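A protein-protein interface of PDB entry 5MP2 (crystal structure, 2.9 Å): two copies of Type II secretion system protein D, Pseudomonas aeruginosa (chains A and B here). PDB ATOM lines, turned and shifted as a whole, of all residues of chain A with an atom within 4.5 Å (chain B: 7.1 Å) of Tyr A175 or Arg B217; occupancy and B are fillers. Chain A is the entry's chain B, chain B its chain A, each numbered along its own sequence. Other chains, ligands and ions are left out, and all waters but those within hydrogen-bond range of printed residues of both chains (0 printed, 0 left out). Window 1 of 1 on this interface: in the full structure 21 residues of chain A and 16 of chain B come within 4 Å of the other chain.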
ATOM      1  N   LEU A 128      17.822  -2.342 -11.254  1.00  0.00           N
ATOM      2  CA  LEU A 128      18.613  -3.429 -10.723  1.00  0.00           C
ATOM      3  C   LEU A 128      18.295  -4.851 -11.208  1.00  0.00           C
ATOM      4  O   LEU A 128      19.113  -5.721 -11.101  1.00  0.00           O
ATOM      5  CB  LEU A 128      18.534  -3.380  -9.211  1.00  0.00           C
ATOM      6  CG  LEU A 128      18.774  -2.029  -8.568  1.00  0.00           C
ATOM      7  CD1 LEU A 128      18.839  -2.190  -7.075  1.00  0.00           C
ATOM      8  CD2 LEU A 128      20.058  -1.409  -9.061  1.00  0.00           C
ATOM      9  N   HIS A 173      18.268   2.061  -2.329  1.00  0.00           N
ATOM     10  CA  HIS A 173      19.241   1.327  -3.115  1.00  0.00           C
ATOM     11  C   HIS A 173      20.181   2.249  -3.880  1.00  0.00           C
ATOM     12  O   HIS A 173      20.006   2.497  -5.073  1.00  0.00           O
ATOM     13  CB  HIS A 173      18.563   0.288  -4.028  1.00  0.00           C
ATOM     14  CG  HIS A 173      17.668  -0.657  -3.280  1.00  0.00           C
ATOM     15  ND1 HIS A 173      16.317  -0.373  -3.079  1.00  0.00           N
ATOM     16  CD2 HIS A 173      17.958  -1.830  -2.677  1.00  0.00           C
ATOM     17  CE1 HIS A 173      15.838  -1.385  -2.377  1.00  0.00           C
ATOM     18  NE2 HIS A 173      16.793  -2.283  -2.115  1.00  0.00           N
ATOM     19  N   ASP A 174      21.184   2.761  -3.154  1.00  0.00           N
ATOM     20  CA  ASP A 174      22.273   3.556  -3.703  1.00  0.00           C
ATOM     21  C   ASP A 174      23.289   2.526  -4.249  1.00  0.00           C
ATOM     22  O   ASP A 174      23.640   1.558  -3.558  1.00  0.00           O
ATOM     23  CB  ASP A 174      22.908   4.457  -2.620  1.00  0.00           C
ATOM     24  CG  ASP A 174      22.033   5.588  -2.092  1.00  0.00           C
ATOM     25  OD1 ASP A 174      20.805   5.554  -2.326  1.00  0.00           O
ATOM     26  OD2 ASP A 174      22.581   6.519  -1.449  1.00  0.00           O
ATOM     27  N   TYR A 175      23.721   2.701  -5.493  1.00  0.00           N
ATOM     28  CA  TYR A 175      24.657   1.771  -6.107  1.00  0.00           C
ATOM     29  C   TYR A 175      25.835   2.451  -6.759  1.00  0.00           C
ATOM     30  O   TYR A 175      25.828   3.658  -6.963  1.00  0.00           O
ATOM     31  CB  TYR A 175      23.943   0.849  -7.111  1.00  0.00           C
ATOM     32  CG  TYR A 175      23.134   1.554  -8.186  1.00  0.00           C
ATOM     33  CD1 TYR A 175      23.739   2.005  -9.358  1.00  0.00           C
ATOM     34  CD2 TYR A 175      21.754   1.698  -8.070  1.00  0.00           C
ATOM     35  CE1 TYR A 175      22.995   2.627 -10.364  1.00  0.00           C
ATOM     36  CE2 TYR A 175      21.001   2.325  -9.065  1.00  0.00           C
ATOM     37  CZ  TYR A 175      21.628   2.789 -10.212  1.00  0.00           C
ATOM     38  OH  TYR A 175      20.895   3.393 -11.205  1.00  0.00           O
ATOM     39  N   SER A 176      26.855   1.668  -7.077  1.00  0.00           N
ATOM     40  CA  SER A 176      28.033   2.101  -7.813  1.00  0.00           C
ATOM     41  C   SER A 176      28.081   1.216  -9.039  1.00  0.00           C
ATOM     42  O   SER A 176      27.859   0.005  -8.947  1.00  0.00           O
ATOM     43  CB  SER A 176      29.310   1.924  -7.000  1.00  0.00           C
ATOM     44  OG  SER A 176      29.361   2.773  -5.866  1.00  0.00           O
ATOM     45  N   VAL A 177      28.326   1.825 -10.189  1.00  0.00           N
ATOM     46  CA  VAL A 177      28.406   1.146 -11.480  1.00  0.00           C
ATOM     47  C   VAL A 177      29.860   1.116 -11.940  1.00  0.00           C
ATOM     48  O   VAL A 177      30.515   2.159 -11.967  1.00  0.00           O
ATOM     49  CB  VAL A 177      27.452   1.796 -12.513  1.00  0.00           C
ATOM     50  CG1 VAL A 177      27.746   1.324 -13.931  1.00  0.00           C
ATOM     51  CG2 VAL A 177      25.994   1.507 -12.162  1.00  0.00           C
ATOM     52  N   ILE A 219      26.926  -3.691 -11.033  1.00  0.00           N
ATOM     53  CA  ILE A 219      26.112  -2.810 -10.220  1.00  0.00           C
ATOM     54  C   ILE A 219      26.378  -3.325  -8.819  1.00  0.00           C
ATOM     55  O   ILE A 219      25.988  -4.442  -8.506  1.00  0.00           O
ATOM     56  CB  ILE A 219      24.618  -2.908 -10.633  1.00  0.00           C
ATOM     57  CG1 ILE A 219      24.399  -2.377 -12.046  1.00  0.00           C
ATOM     58  CG2 ILE A 219      23.725  -2.153  -9.645  1.00  0.00           C
ATOM     59  CD1 ILE A 219      23.114  -2.673 -12.548  1.00  0.00           C
ATOM     60  N   ILE A 220      27.132  -2.559  -8.022  1.00  0.00           N
ATOM     61  CA  ILE A 220      27.527  -2.914  -6.663  1.00  0.00           C
ATOM     62  C   ILE A 220      26.560  -2.240  -5.707  1.00  0.00           C
ATOM     63  O   ILE A 220      26.420  -1.033  -5.764  1.00  0.00           O
ATOM     64  CB  ILE A 220      29.008  -2.478  -6.425  1.00  0.00           C
ATOM     65  CG1 ILE A 220      29.985  -3.037  -7.507  1.00  0.00           C
ATOM     66  CG2 ILE A 220      29.487  -2.802  -4.999  1.00  0.00           C
ATOM     67  CD1 ILE A 220      30.224  -4.625  -7.586  1.00  0.00           C
ATOM     68  N   LEU A 221      25.893  -3.013  -4.837  1.00  0.00           N
ATOM     69  CA  LEU A 221      24.872  -2.537  -3.887  1.00  0.00           C
ATOM     70  C   LEU A 221      25.233  -2.780  -2.439  1.00  0.00           C
ATOM     71  O   LEU A 221      26.322  -3.271  -2.170  1.00  0.00           O
ATOM     72  CB  LEU A 221      23.530  -3.207  -4.189  1.00  0.00           C
ATOM     73  CG  LEU A 221      22.890  -2.872  -5.526  1.00  0.00           C
ATOM     74  CD1 LEU A 221      21.703  -3.704  -5.700  1.00  0.00           C
ATOM     75  CD2 LEU A 221      22.468  -1.421  -5.585  1.00  0.00           C
ATOM     76  N   ARG A 227      29.838  -1.551   0.239  1.00  0.00           N
ATOM     77  CA  ARG A 227      29.793  -1.241  -1.189  1.00  0.00           C
ATOM     78  C   ARG A 227      31.100  -0.629  -1.712  1.00  0.00           C
ATOM     79  O   ARG A 227      31.493  -0.946  -2.826  1.00  0.00           O
ATOM     80  CB  ARG A 227      28.575  -0.341  -1.467  1.00  0.00           C
ATOM     81  CG  ARG A 227      28.466   0.229  -2.879  1.00  0.00           C
ATOM     82  CD  ARG A 227      27.074   0.726  -3.283  1.00  0.00           C
ATOM     83  NE  ARG A 227      26.293   1.422  -2.245  1.00  0.00           N
ATOM     84  CZ  ARG A 227      26.594   2.611  -1.722  1.00  0.00           C
ATOM     85  NH1 ARG A 227      25.794   3.168  -0.827  1.00  0.00           N
ATOM     86  NH2 ARG A 227      27.714   3.234  -2.068  1.00  0.00           N
ATOM     87  N   PRO B 127      22.858   4.855 -19.991  1.00  0.00           N
ATOM     88  CA  PRO B 127      22.361   4.889 -18.627  1.00  0.00           C
ATOM     89  C   PRO B 127      22.445   6.246 -18.035  1.00  0.00           C
ATOM     90  O   PRO B 127      21.596   6.624 -17.283  1.00  0.00           O
ATOM     91  CB  PRO B 127      23.290   3.931 -17.915  1.00  0.00           C
ATOM     92  CG  PRO B 127      23.581   2.920 -18.943  1.00  0.00           C
ATOM     93  CD  PRO B 127      23.804   3.748 -20.168  1.00  0.00           C
ATOM     94  N   ARG B 130      19.590   8.293 -20.096  1.00  0.00           N
ATOM     95  CA  ARG B 130      18.195   7.886 -19.869  1.00  0.00           C
ATOM     96  C   ARG B 130      17.496   8.738 -18.789  1.00  0.00           C
ATOM     97  O   ARG B 130      16.402   9.221 -19.085  1.00  0.00           O
ATOM     98  CB  ARG B 130      18.042   6.374 -19.603  1.00  0.00           C
ATOM     99  N   PRO B 131      18.136   9.063 -17.624  1.00  0.00           N
ATOM    100  CA  PRO B 131      17.474   9.928 -16.625  1.00  0.00           C
ATOM    101  C   PRO B 131      17.036  11.307 -17.125  1.00  0.00           C
ATOM    102  O   PRO B 131      16.182  11.938 -16.498  1.00  0.00           O
ATOM    103  CB  PRO B 131      18.540  10.067 -15.540  1.00  0.00           C
ATOM    104  CG  PRO B 131      19.326   8.820 -15.643  1.00  0.00           C
ATOM    105  CD  PRO B 131      19.446   8.607 -17.107  1.00  0.00           C
ATOM    106  N   TYR B 175      30.082   5.454 -12.360  1.00  0.00           N
ATOM    107  CA  TYR B 175      29.302   6.452 -11.637  1.00  0.00           C
ATOM    108  C   TYR B 175      28.655   5.924 -10.360  1.00  0.00           C
ATOM    109  O   TYR B 175      28.436   4.726 -10.258  1.00  0.00           O
ATOM    110  CB  TYR B 175      28.243   7.031 -12.585  1.00  0.00           C
ATOM    111  CG  TYR B 175      27.211   6.038 -13.096  1.00  0.00           C
ATOM    112  CD1 TYR B 175      27.377   5.400 -14.325  1.00  0.00           C
ATOM    113  CD2 TYR B 175      26.031   5.803 -12.396  1.00  0.00           C
ATOM    114  CE1 TYR B 175      26.390   4.557 -14.841  1.00  0.00           C
ATOM    115  CE2 TYR B 175      25.056   4.935 -12.884  1.00  0.00           C
ATOM    116  CZ  TYR B 175      25.237   4.318 -14.109  1.00  0.00           C
ATOM    117  OH  TYR B 175      24.274   3.455 -14.565  1.00  0.00           O
ATOM    118  N   SER B 176      28.304   6.811  -9.414  1.00  0.00           N
ATOM    119  CA  SER B 176      27.618   6.475  -8.153  1.00  0.00           C
ATOM    120  C   SER B 176      26.240   7.132  -8.186  1.00  0.00           C
ATOM    121  O   SER B 176      26.139   8.300  -8.561  1.00  0.00           O
ATOM    122  CB  SER B 176      28.390   7.004  -6.944  1.00  0.00           C
ATOM    123  OG  SER B 176      29.689   6.454  -6.799  1.00  0.00           O
ATOM    124  N   VAL B 177      25.191   6.392  -7.792  1.00  0.00           N
ATOM    125  CA  VAL B 177      23.803   6.874  -7.721  1.00  0.00           C
ATOM    126  C   VAL B 177      23.424   7.088  -6.261  1.00  0.00           C
ATOM    127  O   VAL B 177      23.596   6.174  -5.449  1.00  0.00           O
ATOM    128  CB  VAL B 177      22.810   5.951  -8.489  1.00  0.00           C
ATOM    129  CG1 VAL B 177      21.349   6.287  -8.171  1.00  0.00           C
ATOM    130  CG2 VAL B 177      23.071   6.032  -9.991  1.00  0.00           C
ATOM    131  N   ILE B 178      22.950   8.308  -5.927  1.00  0.00           N
ATOM    132  CA  ILE B 178      22.545   8.678  -4.566  1.00  0.00           C
ATOM    133  C   ILE B 178      21.065   9.034  -4.519  1.00  0.00           C
ATOM    134  O   ILE B 178      20.699  10.136  -4.920  1.00  0.00           O
ATOM    135  CB  ILE B 178      23.411   9.846  -3.996  1.00  0.00           C
ATOM    136  CG1 ILE B 178      24.899   9.549  -4.111  1.00  0.00           C
ATOM    137  CG2 ILE B 178      23.027  10.189  -2.543  1.00  0.00           C
ATOM    138  CD1 ILE B 178      25.761  10.786  -4.187  1.00  0.00           C
ATOM    139  N   ASN B 179      20.228   8.127  -4.000  1.00  0.00           N
ATOM    140  CA  ASN B 179      18.806   8.413  -3.839  1.00  0.00           C
ATOM    141  C   ASN B 179      18.662   9.325  -2.602  1.00  0.00           C
ATOM    142  O   ASN B 179      19.098   8.937  -1.513  1.00  0.00           O
ATOM    143  CB  ASN B 179      17.999   7.110  -3.733  1.00  0.00           C
ATOM    144  CG  ASN B 179      17.895   6.339  -5.041  1.00  0.00           C
ATOM    145  OD1 ASN B 179      17.257   6.781  -6.009  1.00  0.00           O
ATOM    146  ND2 ASN B 179      18.505   5.159  -5.104  1.00  0.00           N
ATOM    147  N   LEU B 180      18.176  10.583  -2.804  1.00  0.00           N
ATOM    148  CA  LEU B 180      18.029  11.606  -1.754  1.00  0.00           C
ATOM    149  C   LEU B 180      16.692  11.494  -1.027  1.00  0.00           C
ATOM    150  O   LEU B 180      15.631  11.569  -1.668  1.00  0.00           O
ATOM    151  CB  LEU B 180      18.229  13.034  -2.306  1.00  0.00           C
ATOM    152  CG  LEU B 180      19.622  13.424  -2.789  1.00  0.00           C
ATOM    153  CD1 LEU B 180      19.620  14.796  -3.352  1.00  0.00           C
ATOM    154  CD2 LEU B 180      20.619  13.372  -1.685  1.00  0.00           C
ATOM    155  N   VAL B 185      16.983  17.167  -5.059  1.00  0.00           N
ATOM    156  CA  VAL B 185      18.012  16.846  -6.037  1.00  0.00           C
ATOM    157  C   VAL B 185      18.606  18.103  -6.682  1.00  0.00           C
ATOM    158  O   VAL B 185      19.824  18.241  -6.672  1.00  0.00           O
ATOM    159  CB  VAL B 185      17.529  15.804  -7.071  1.00  0.00           C
ATOM    160  CG1 VAL B 185      16.428  16.361  -7.967  1.00  0.00           C
ATOM    161  CG2 VAL B 185      18.688  15.280  -7.900  1.00  0.00           C
ATOM    162  N   MET B 186      17.762  19.031  -7.188  1.00  0.00           N
ATOM    163  CA  MET B 186      18.218  20.247  -7.876  1.00  0.00           C
ATOM    164  C   MET B 186      18.972  21.216  -6.980  1.00  0.00           C
ATOM    165  O   MET B 186      19.789  21.988  -7.487  1.00  0.00           O
ATOM    166  CB  MET B 186      17.076  20.958  -8.599  1.00  0.00           C
ATOM    167  CG  MET B 186      16.465  20.155  -9.723  1.00  0.00           C
ATOM    168  SD  MET B 186      17.595  19.570 -11.045  1.00  0.00           S
ATOM    169  CE  MET B 186      18.798  20.973 -11.242  1.00  0.00           C
ATOM    170  N   ALA B 189      22.429  19.278  -6.539  1.00  0.00           N
ATOM    171  CA  ALA B 189      23.155  19.334  -7.808  1.00  0.00           C
ATOM    172  C   ALA B 189      23.782  20.723  -7.990  1.00  0.00           C
ATOM    173  O   ALA B 189      24.982  20.799  -8.262  1.00  0.00           O
ATOM    174  CB  ALA B 189      22.232  19.001  -8.972  1.00  0.00           C
ATOM    175  N   VAL B 209      27.934  16.023 -12.208  1.00  0.00           N
ATOM    176  CA  VAL B 209      26.714  15.764 -11.480  1.00  0.00           C
ATOM    177  C   VAL B 209      25.576  15.805 -12.493  1.00  0.00           C
ATOM    178  O   VAL B 209      25.431  16.792 -13.223  1.00  0.00           O
ATOM    179  CB  VAL B 209      26.447  16.662 -10.220  1.00  0.00           C
ATOM    180  CG1 VAL B 209      25.075  16.372  -9.617  1.00  0.00           C
ATOM    181  CG2 VAL B 209      27.520  16.479  -9.158  1.00  0.00           C
ATOM    182  N   ILE B 210      24.783  14.713 -12.517  1.00  0.00           N
ATOM    183  CA  ILE B 210      23.583  14.553 -13.326  1.00  0.00           C
ATOM    184  C   ILE B 210      22.428  14.413 -12.323  1.00  0.00           C
ATOM    185  O   ILE B 210      22.471  13.517 -11.487  1.00  0.00           O
ATOM    186  CB  ILE B 210      23.687  13.356 -14.311  1.00  0.00           C
ATOM    187  CG1 ILE B 210      24.838  13.558 -15.318  1.00  0.00           C
ATOM    188  CG2 ILE B 210      22.341  13.132 -15.000  1.00  0.00           C
ATOM    189  CD1 ILE B 210      25.052  12.483 -16.408  1.00  0.00           C
ATOM    190  N   ALA B 211      21.437  15.337 -12.362  1.00  0.00           N
ATOM    191  CA  ALA B 211      20.293  15.360 -11.432  1.00  0.00           C
ATOM    192  C   ALA B 211      19.038  14.733 -12.042  1.00  0.00           C
ATOM    193  O   ALA B 211      18.509  15.249 -13.024  1.00  0.00           O
ATOM    194  CB  ALA B 211      20.005  16.776 -10.949  1.00  0.00           C
ATOM    195  N   ASP B 212      18.551  13.635 -11.451  1.00  0.00           N
ATOM    196  CA  ASP B 212      17.346  12.962 -11.908  1.00  0.00           C
ATOM    197  C   ASP B 212      16.207  13.403 -10.967  1.00  0.00           C
ATOM    198  O   ASP B 212      16.040  12.854  -9.872  1.00  0.00           O
ATOM    199  CB  ASP B 212      17.536  11.422 -11.964  1.00  0.00           C
ATOM    200  CG  ASP B 212      16.367  10.638 -12.531  1.00  0.00           C
ATOM    201  OD1 ASP B 212      15.379  11.272 -12.998  1.00  0.00           O
ATOM    202  OD2 ASP B 212      16.440   9.399 -12.538  1.00  0.00           O
ATOM    203  N   ALA B 213      15.449  14.434 -11.389  1.00  0.00           N
ATOM    204  CA  ALA B 213      14.367  14.993 -10.594  1.00  0.00           C
ATOM    205  C   ALA B 213      13.257  13.989 -10.415  1.00  0.00           C
ATOM    206  O   ALA B 213      12.775  13.837  -9.292  1.00  0.00           O
ATOM    207  CB  ALA B 213      13.861  16.259 -11.222  1.00  0.00           C
ATOM    208  N   ARG B 214      12.922  13.233 -11.500  1.00  0.00           N
ATOM    209  CA  ARG B 214      11.872  12.209 -11.538  1.00  0.00           C
ATOM    210  C   ARG B 214      11.950  11.194 -10.376  1.00  0.00           C
ATOM    211  O   ARG B 214      10.905  10.805  -9.845  1.00  0.00           O
ATOM    212  CB  ARG B 214      11.841  11.503 -12.902  1.00  0.00           C
ATOM    213  N   THR B 215      13.168  10.918  -9.930  1.00  0.00           N
ATOM    214  CA  THR B 215      13.433   9.943  -8.901  1.00  0.00           C
ATOM    215  C   THR B 215      14.207  10.461  -7.716  1.00  0.00           C
ATOM    216  O   THR B 215      14.519   9.711  -6.810  1.00  0.00           O
ATOM    217  CB  THR B 215      14.228   8.816  -9.508  1.00  0.00           C
ATOM    218  OG1 THR B 215      15.294   9.386 -10.248  1.00  0.00           O
ATOM    219  CG2 THR B 215      13.390   8.087 -10.478  1.00  0.00           C
ATOM    220  N   ASN B 216      14.495  11.750  -7.737  1.00  0.00           N
ATOM    221  CA  ASN B 216      15.222  12.472  -6.695  1.00  0.00           C
ATOM    222  C   ASN B 216      16.609  12.010  -6.402  1.00  0.00           C
ATOM    223  O   ASN B 216      17.001  11.971  -5.278  1.00  0.00           O
ATOM    224  CB  ASN B 216      14.441  12.587  -5.399  1.00  0.00           C
ATOM    225  CG  ASN B 216      14.562  13.944  -4.778  1.00  0.00           C
ATOM    226  OD1 ASN B 216      14.312  14.941  -5.414  1.00  0.00           O
ATOM    227  ND2 ASN B 216      14.916  13.983  -3.522  1.00  0.00           N
ATOM    228  N   ARG B 217      17.391  11.732  -7.422  1.00  0.00           N
ATOM    229  CA  ARG B 217      18.731  11.287  -7.182  1.00  0.00           C
ATOM    230  C   ARG B 217      19.775  11.939  -8.018  1.00  0.00           C
ATOM    231  O   ARG B 217      19.510  12.505  -9.033  1.00  0.00           O
ATOM    232  CB  ARG B 217      18.818   9.794  -7.362  1.00  0.00           C
ATOM    233  CG  ARG B 217      18.815   9.345  -8.784  1.00  0.00           C
ATOM    234  CD  ARG B 217      17.953   8.123  -8.945  1.00  0.00           C
ATOM    235  NE  ARG B 217      17.778   7.835 -10.352  1.00  0.00           N
ATOM    236  CZ  ARG B 217      18.333   6.812 -10.966  1.00  0.00           C
ATOM    237  NH1 ARG B 217      18.145   6.610 -12.245  1.00  0.00           N
ATOM    238  NH2 ARG B 217      19.061   5.984 -10.284  1.00  0.00           N
ATOM    239  N   LEU B 218      20.992  11.842  -7.533  1.00  0.00           N
ATOM    240  CA  LEU B 218      22.145  12.383  -8.172  1.00  0.00           C
ATOM    241  C   LEU B 218      23.005  11.265  -8.655  1.00  0.00           C
ATOM    242  O   LEU B 218      23.219  10.305  -7.963  1.00  0.00           O
ATOM    243  CB  LEU B 218      22.973  13.096  -7.152  1.00  0.00           C
ATOM    244  CG  LEU B 218      22.436  14.330  -6.517  1.00  0.00           C
ATOM    245  CD1 LEU B 218      23.374  14.602  -5.375  1.00  0.00           C
ATOM    246  CD2 LEU B 218      22.532  15.425  -7.541  1.00  0.00           C
ATOM    247  N   ILE B 219      23.513  11.408  -9.854  1.00  0.00           N
ATOM    248  CA  ILE B 219      24.406  10.448 -10.399  1.00  0.00           C
ATOM    249  C   ILE B 219      25.719  11.144 -10.311  1.00  0.00           C
ATOM    250  O   ILE B 219      25.851  12.216 -10.829  1.00  0.00           O
ATOM    251  CB  ILE B 219      24.154  10.277 -11.867  1.00  0.00           C
ATOM    252  CG1 ILE B 219      22.797   9.672 -12.122  1.00  0.00           C
ATOM    253  CG2 ILE B 219      25.176   9.362 -12.445  1.00  0.00           C
ATOM    254  CD1 ILE B 219      22.403   9.730 -13.575  1.00  0.00           C
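The backbone carbonyl oxygen (O) of Tyr B175 lies within hydrogen-bond range of the backbone NH (N) of Val A177 (2.9 Å). N of Val B177 is in hydrogen-bond range of O of Tyr A175, at 2.9 Å. The side-chain amide nitrogen (ND2) of Asn B179 is in hydrogen-bond range of the backbone carbonyl oxygen (O) of His A173, 3.1 Å away. The side-chain carboxylate of Asp A174 sits at hydrogen-bond distance from the backbone NH of Asn B179. NH2 of Arg B217 sits at hydrogen-bond distance from OH of Tyr A175 (3.3 Å).
N of Ile B178 sits at hydrogen-bond distance from O of Leu B218, at 2.9 Å. The side-chain carboxylate of Asp B212 lies within salt-bridge range of the guanidinium group of Arg B217, at 3.0 Å. OG1 of Thr B215 is in hydrogen-bond range of NE of Arg B217. O of Asp A174 lies within hydrogen-bond range of NE of Arg A227 (3.0 Å). The backbone carbonyl oxygen (O) of Ser A176 sits at hydrogen-bond distance from the backbone NH (N) of Ile A220.
O of Val B177 touches CB of Asp A174, 3.4 Å away. Asp A174 touches Ile B178 (OD2 to CA, 3.8 Å). Tyr A175 touches Tyr B175. CA of Ser B176 touches O of Tyr A175 (3.5 Å). CA of Ser A176 touches O of Tyr B175, 3.6 Å away. Ser B176 touches Ser A176 (OG to OG, 3.8 Å).
Of the printed residues of chain B, Tyr A175 touches Tyr B175, Ser B176, Val B177 and Arg B217. Printed residues of chain A within 4 Å of Tyr B175: Tyr A175 (3.99 Å), Ser A176 (3.6 Å) and Val A177 (2.9 Å). Printed residues of chain A within 4 Å of Ile B178: Asp A174. Of chain A, only Tyr A175 comes within 4 Å of Arg B217. The nearest printed residue of chain A that does not touch Ser B176 is Val A177 (5.0 Å).
Of the 23 printed residues of chain B, 6 touch a printed residue of chain A. Printed residues of chain B that touch a printed residue of chain A: Tyr B175, Ser B176, Val B177, Ile B178, Asn B179 and Arg B217. Printed residues of chain A that touch a printed residue of chain B: His A173, Asp A174, Tyr A175, Ser A176 and Val A177. Among the printed residues, no Asp or Glu carboxylate lies within 4 Å of a Lys or Arg side-chain nitrogen of the other chain.
Tyr B175 touches its own counterpart, Tyr A175. Tyr A175 touches Ser B176, and with the chains exchanged Ser A176 touches Tyr B175. Tyr A175 touches Val B177, and with the chains exchanged Val A177 touches Tyr B175. Ser B176 touches its own counterpart, Ser A176.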
